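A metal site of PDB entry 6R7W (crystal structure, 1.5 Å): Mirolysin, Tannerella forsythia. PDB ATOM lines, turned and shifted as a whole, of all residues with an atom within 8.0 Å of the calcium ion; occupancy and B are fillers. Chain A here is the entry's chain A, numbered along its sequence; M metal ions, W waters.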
ATOM      1  N   HIS A 180      20.990  14.964   8.246  1.00  0.00           N
ATOM      2  CA  HIS A 180      20.451  15.659   7.068  1.00  0.00           C
ATOM      3  C   HIS A 180      19.052  16.149   7.332  1.00  0.00           C
ATOM      4  O   HIS A 180      18.203  15.408   7.838  1.00  0.00           O
ATOM      5  CB  HIS A 180      20.465  14.734   5.879  1.00  0.00           C
ATOM      6  CG  HIS A 180      21.852  14.541   5.383  1.00  0.00           C
ATOM      7  ND1 HIS A 180      22.257  13.340   4.843  1.00  0.00           N
ATOM      8  CD2 HIS A 180      22.910  15.380   5.434  1.00  0.00           C
ATOM      9  CE1 HIS A 180      23.527  13.499   4.523  1.00  0.00           C
ATOM     10  NE2 HIS A 180      23.979  14.706   4.878  1.00  0.00           N
ATOM     11  N   ILE A 181      18.802  17.401   6.941  1.00  0.00           N
ATOM     12  CA  ILE A 181      17.521  18.051   7.242  1.00  0.00           C
ATOM     13  C   ILE A 181      16.334  17.303   6.595  1.00  0.00           C
ATOM     14  O   ILE A 181      15.238  17.329   7.167  1.00  0.00           O
ATOM     15  CB  ILE A 181      17.617  19.547   6.823  1.00  0.00           C
ATOM     16  CG1 ILE A 181      16.399  20.313   7.317  1.00  0.00           C
ATOM     17  CG2 ILE A 181      17.871  19.770   5.304  1.00  0.00           C
ATOM     18  CD1 ILE A 181      16.619  21.841   7.251  1.00  0.00           C
ATOM     19  N   TRP A 182      16.555  16.612   5.478  1.00  0.00           N
ATOM     20  CA  TRP A 182      15.464  15.902   4.795  1.00  0.00           C
ATOM     21  C   TRP A 182      15.214  14.502   5.396  1.00  0.00           C
ATOM     22  O   TRP A 182      14.269  13.819   4.993  1.00  0.00           O
ATOM     23  CB  TRP A 182      15.707  15.813   3.285  1.00  0.00           C
ATOM     24  CG  TRP A 182      16.830  14.918   2.898  1.00  0.00           C
ATOM     25  CD1 TRP A 182      16.742  13.598   2.532  1.00  0.00           C
ATOM     26  CD2 TRP A 182      18.209  15.278   2.789  1.00  0.00           C
ATOM     27  NE1 TRP A 182      17.990  13.106   2.256  1.00  0.00           N
ATOM     28  CE2 TRP A 182      18.912  14.111   2.411  1.00  0.00           C
ATOM     29  CE3 TRP A 182      18.917  16.474   2.974  1.00  0.00           C
ATOM     30  CZ2 TRP A 182      20.297  14.118   2.185  1.00  0.00           C
ATOM     31  CZ3 TRP A 182      20.292  16.478   2.758  1.00  0.00           C
ATOM     32  CH2 TRP A 182      20.969  15.322   2.365  1.00  0.00           C
ATOM     33  N   GLY A 183      16.049  14.066   6.332  1.00  0.00           N
ATOM     34  CA  GLY A 183      15.786  12.777   6.977  1.00  0.00           C
ATOM     35  C   GLY A 183      16.289  11.508   6.316  1.00  0.00           C
ATOM     36  O   GLY A 183      15.903  10.418   6.756  1.00  0.00           O
ATOM     37  N   ASP A 184      17.105  11.617   5.228  1.00  0.00           N
ATOM     38  CA  ASP A 184      17.769  10.458   4.574  1.00  0.00           C
ATOM     39  C   ASP A 184      16.756   9.381   4.216  1.00  0.00           C
ATOM     40  O   ASP A 184      16.962   8.186   4.491  1.00  0.00           O
ATOM     41  CB  ASP A 184      18.843   9.883   5.508  1.00  0.00           C
ATOM     42  CG  ASP A 184      19.924  10.893   5.747  1.00  0.00           C
ATOM     43  OD1 ASP A 184      20.546  11.320   4.770  1.00  0.00           O
ATOM     44  OD2 ASP A 184      20.124  11.271   6.907  1.00  0.00           O
ATOM     45  N   ASP A 185      15.670   9.807   3.615  1.00  0.00           N
ATOM     46  CA  ASP A 185      14.565   8.914   3.306  1.00  0.00           C
ATOM     47  C   ASP A 185      14.174   8.963   1.812  1.00  0.00           C
ATOM     48  O   ASP A 185      13.052   8.609   1.436  1.00  0.00           O
ATOM     49  CB  ASP A 185      13.393   9.288   4.211  1.00  0.00           C
ATOM     50  CG  ASP A 185      12.958  10.734   4.035  1.00  0.00           C
ATOM     51  OD1 ASP A 185      13.446  11.404   3.109  1.00  0.00           O
ATOM     52  OD2 ASP A 185      12.137  11.199   4.829  1.00  0.00           O
ATOM     53  N   GLY A 186      15.110   9.449   0.987  1.00  0.00           N
ATOM     54  CA  GLY A 186      14.954   9.488  -0.473  1.00  0.00           C
ATOM     55  C   GLY A 186      13.822  10.294  -1.054  1.00  0.00           C
ATOM     56  O   GLY A 186      13.391  10.023  -2.180  1.00  0.00           O
ATOM     57  N   GLY A 187      13.335  11.279  -0.309  1.00  0.00           N
ATOM     58  CA  GLY A 187      12.274  12.140  -0.814  1.00  0.00           C
ATOM     59  C   GLY A 187      10.964  12.025  -0.083  1.00  0.00           C
ATOM     60  O   GLY A 187      10.062  12.839  -0.311  1.00  0.00           O
ATOM     61  N   SER A 188      10.839  11.016   0.811  1.00  0.00           N
ATOM     62  CA  SER A 188       9.576  10.800   1.505  1.00  0.00           C
ATOM     63  C   SER A 188       9.398  11.806   2.656  1.00  0.00           C
ATOM     64  O   SER A 188      10.285  12.618   2.926  1.00  0.00           O
ATOM     65  CB  SER A 188       9.468   9.362   2.007  1.00  0.00           C
ATOM     66  OG  SER A 188      10.213   9.139   3.178  1.00  0.00           O
ATOM     67  N   CYS A 189       8.244  11.762   3.318  1.00  0.00           N
ATOM     68  CA  CYS A 189       7.993  12.666   4.441  1.00  0.00           C
ATOM     69  C   CYS A 189       8.131  11.940   5.764  1.00  0.00           C
ATOM     70  O   CYS A 189       7.937  12.543   6.806  1.00  0.00           O
ATOM     71  CB  CYS A 189       6.628  13.311   4.294  1.00  0.00           C
ATOM     72  SG  CYS A 189       6.476  14.352   2.822  1.00  0.00           S
ATOM     73  N   SER A 190       8.495  10.640   5.746  1.00  0.00           N
ATOM     74  CA  SER A 190       8.477   9.845   6.985  1.00  0.00           C
ATOM     75  C   SER A 190       9.781   9.822   7.761  1.00  0.00           C
ATOM     76  O   SER A 190       9.743   9.578   8.972  1.00  0.00           O
ATOM     77  CB  SER A 190       8.040   8.423   6.678  1.00  0.00           C
ATOM     78  OG  SER A 190       8.878   7.861   5.694  1.00  0.00           O
ATOM     79  N   GLY A 191      10.907  10.136   7.112  1.00  0.00           N
ATOM     80  CA  GLY A 191      12.164  10.241   7.817  1.00  0.00           C
ATOM     81  C   GLY A 191      12.220  11.561   8.572  1.00  0.00           C
ATOM     82  O   GLY A 191      11.387  12.437   8.368  1.00  0.00           O
ATOM     83  N   THR A 192      13.153  11.656   9.506  1.00  0.00           N
ATOM     84  CA  THR A 192      13.262  12.844  10.337  1.00  0.00           C
ATOM     85  C   THR A 192      14.707  13.160  10.626  1.00  0.00           C
ATOM     86  O   THR A 192      15.554  12.276  10.626  1.00  0.00           O
ATOM     87  CB  THR A 192      12.487  12.602  11.673  1.00  0.00           C
ATOM     88  OG1 THR A 192      12.505  13.791  12.462  1.00  0.00           O
ATOM     89  CG2 THR A 192      13.034  11.419  12.500  1.00  0.00           C
ATOM     90  N   ASP A 193      14.974  14.440  10.940  1.00  0.00           N
ATOM     91  CA  ASP A 193      16.302  14.797  11.417  1.00  0.00           C
ATOM     92  C   ASP A 193      16.243  14.957  12.938  1.00  0.00           C
ATOM     93  O   ASP A 193      17.236  15.335  13.577  1.00  0.00           O
ATOM     94  CB  ASP A 193      16.858  16.075  10.732  1.00  0.00           C
ATOM     95  CG  ASP A 193      16.093  17.362  10.992  1.00  0.00           C
ATOM     96  OD1 ASP A 193      14.914  17.278  11.444  1.00  0.00           O
ATOM     97  OD2 ASP A 193      16.665  18.451  10.754  1.00  0.00           O
ATOM     98  N   PRO A 199      11.753  22.480   9.220  1.00  0.00           N
ATOM     99  CA  PRO A 199      10.505  21.981   8.598  1.00  0.00           C
ATOM    100  C   PRO A 199      10.691  20.599   7.965  1.00  0.00           C
ATOM    101  O   PRO A 199      11.741  20.334   7.351  1.00  0.00           O
ATOM    102  CB  PRO A 199      10.186  23.040   7.546  1.00  0.00           C
ATOM    103  CG  PRO A 199      10.901  24.287   7.977  1.00  0.00           C
ATOM    104  CD  PRO A 199      12.149  23.810   8.692  1.00  0.00           C
ATOM    105  N   ASN A 200       9.679  19.752   8.062  1.00  0.00           N
ATOM    106  CA  ASN A 200       9.760  18.438   7.419  1.00  0.00           C
ATOM    107  C   ASN A 200      10.024  18.654   5.919  1.00  0.00           C
ATOM    108  O   ASN A 200       9.451  19.545   5.298  1.00  0.00           O
ATOM    109  CB  ASN A 200       8.483  17.664   7.651  1.00  0.00           C
ATOM    110  CG  ASN A 200       8.635  16.208   7.305  1.00  0.00           C
ATOM    111  OD1 ASN A 200       9.744  15.715   7.101  1.00  0.00           O
ATOM    112  ND2 ASN A 200       7.503  15.488   7.226  1.00  0.00           N
ATOM    113  N   GLN A 201      10.942  17.875   5.369  1.00  0.00           N
ATOM    114  CA  GLN A 201      11.413  18.085   3.999  1.00  0.00           C
ATOM    115  C   GLN A 201      11.515  16.754   3.312  1.00  0.00           C
ATOM    116  O   GLN A 201      11.897  15.757   3.928  1.00  0.00           O
ATOM    117  CB  GLN A 201      12.787  18.785   4.109  1.00  0.00           C
ATOM    118  CG  GLN A 201      13.482  19.087   2.785  1.00  0.00           C
ATOM    119  CD  GLN A 201      14.771  19.844   3.025  1.00  0.00           C
ATOM    120  OE1 GLN A 201      14.852  20.723   3.869  1.00  0.00           O
ATOM    121  NE2 GLN A 201      15.807  19.537   2.264  1.00  0.00           N
ATOM    122  N   GLY A 202      11.146  16.731   2.040  1.00  0.00           N
ATOM    123  CA  GLY A 202      11.139  15.514   1.246  1.00  0.00           C
ATOM    124  C   GLY A 202      12.540  14.997   1.008  1.00  0.00           C
ATOM    125  O   GLY A 202      13.029  14.125   1.734  1.00  0.00           O
ATOM    126  N   GLY A 203      13.187  15.554  -0.007  1.00  0.00           N
ATOM    127  CA  GLY A 203      14.553  15.162  -0.334  1.00  0.00           C
ATOM    128  C   GLY A 203      15.548  16.280  -0.179  1.00  0.00           C
ATOM    129  O   GLY A 203      15.206  17.391   0.240  1.00  0.00           O
ATOM    130  N   TYR A 204      16.809  16.023  -0.553  1.00  0.00           N
ATOM    131  CA  TYR A 204      17.795  17.095  -0.460  1.00  0.00           C
ATOM    132  C   TYR A 204      17.579  18.157  -1.539  1.00  0.00           C
ATOM    133  O   TYR A 204      16.970  17.929  -2.592  1.00  0.00           O
ATOM    134  CB  TYR A 204      19.233  16.548  -0.564  1.00  0.00           C
ATOM    135  CG  TYR A 204      19.586  15.846  -1.855  1.00  0.00           C
ATOM    136  CD1 TYR A 204      19.711  14.460  -1.893  1.00  0.00           C
ATOM    137  CD2 TYR A 204      19.907  16.568  -3.004  1.00  0.00           C
ATOM    138  CE1 TYR A 204      20.105  13.811  -3.058  1.00  0.00           C
ATOM    139  CE2 TYR A 204      20.281  15.923  -4.177  1.00  0.00           C
ATOM    140  CZ  TYR A 204      20.366  14.538  -4.205  1.00  0.00           C
ATOM    141  OH  TYR A 204      20.758  13.893  -5.361  1.00  0.00           O
ATOM    142  N   ASP A 215       7.356  21.748  -0.618  1.00  0.00           N
ATOM    143  CA  ASP A 215       7.409  20.394  -1.156  1.00  0.00           C
ATOM    144  C   ASP A 215       6.224  19.617  -0.552  1.00  0.00           C
ATOM    145  O   ASP A 215       5.400  20.217   0.147  1.00  0.00           O
ATOM    146  CB  ASP A 215       8.777  19.708  -0.962  1.00  0.00           C
ATOM    147  CG  ASP A 215       9.179  19.354   0.462  1.00  0.00           C
ATOM    148  OD1 ASP A 215       8.298  19.384   1.361  1.00  0.00           O
ATOM    149  OD2 ASP A 215      10.337  18.969   0.652  1.00  0.00           O
ATOM    150  N   HIS A 216       6.094  18.316  -0.823  1.00  0.00           N
ATOM    151  CA  HIS A 216       4.925  17.627  -0.296  1.00  0.00           C
ATOM    152  C   HIS A 216       4.928  17.469   1.236  1.00  0.00           C
ATOM    153  O   HIS A 216       3.862  17.241   1.812  1.00  0.00           O
ATOM    154  CB  HIS A 216       4.729  16.261  -0.990  1.00  0.00           C
ATOM    155  CG  HIS A 216       5.792  15.230  -0.759  1.00  0.00           C
ATOM    156  ND1 HIS A 216       5.469  13.892  -0.661  1.00  0.00           N
ATOM    157  CD2 HIS A 216       7.136  15.358  -0.639  1.00  0.00           C
ATOM    158  CE1 HIS A 216       6.619  13.242  -0.510  1.00  0.00           C
ATOM    159  NE2 HIS A 216       7.643  14.085  -0.471  1.00  0.00           N
ATOM    160  N   CYS A 217       6.073  17.673   1.899  1.00  0.00           N
ATOM    161  CA  CYS A 217       6.158  17.591   3.359  1.00  0.00           C
ATOM    162  C   CYS A 217       5.798  18.918   4.046  1.00  0.00           C
ATOM    163  O   CYS A 217       5.169  18.884   5.108  1.00  0.00           O
ATOM    164  CB  CYS A 217       7.544  17.120   3.775  1.00  0.00           C
ATOM    165  SG  CYS A 217       8.096  15.629   2.919  1.00  0.00           S
HETATM  166 CA    CA M   1      12.265  13.396   3.885  1.00  0.00          CA
HETATM  167  O   HOH W   1      11.190  13.796   6.008  1.00  0.00           O
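OG of Ser 188 is in hydrogen-bond range of OG of Ser 190 (3.1 Å).
The side-chain amide nitrogen of Gln 201 sits at hydrogen-bond distance from the backbone carbonyl oxygen of Gly 203 (3.0 Å).
The side-chain carboxylate of Asp 185 lies close to the backbone NH of Gly 187 (3.4 Å).
The backbone NH (N) of Gly 191 lies close to the side-chain carboxylate (OD2) of Asp 185, at 2.8 Å.
N of Gly 202 is in hydrogen-bond range of SG of Cys 217 (3.4 Å).
The side-chain carboxylate of Asp 215 is in hydrogen-bond range of the backbone NH of Gly 202.
The side-chain sulfur (SG) of Cys 217 is disulfide-bonded to the side-chain sulfur (SG) of Cys 189, 2.1 Å away.
Of the 23 residues printed, 5 come within 4 Å of the calcium ion.
The nearest printed residue that does not touch the calcium ion is Cys 189 (4.4 Å).
O of Trp 182 binds the calcium ion (2.3 Å).
The backbone carbonyl oxygen (O) of Ser 188 binds the calcium ion, at 2.3 Å.
O of Gln 201 is bound to the calcium ion (2.4 Å).
OD2 of Asp 185 binds the calcium ion (2.4 Å).
O of Gly 202 is bound to the calcium ion (2.4 Å).
Water W1 binds the calcium ion (2.4 Å).
The calcium ion is bound by the side-chain carboxylate (OD1) of Asp 185, 2.4 Å away.
Water W1 bridges OD1 of Asn 200 (2.6 Å) and O of Gly 191 (2.7 Å).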
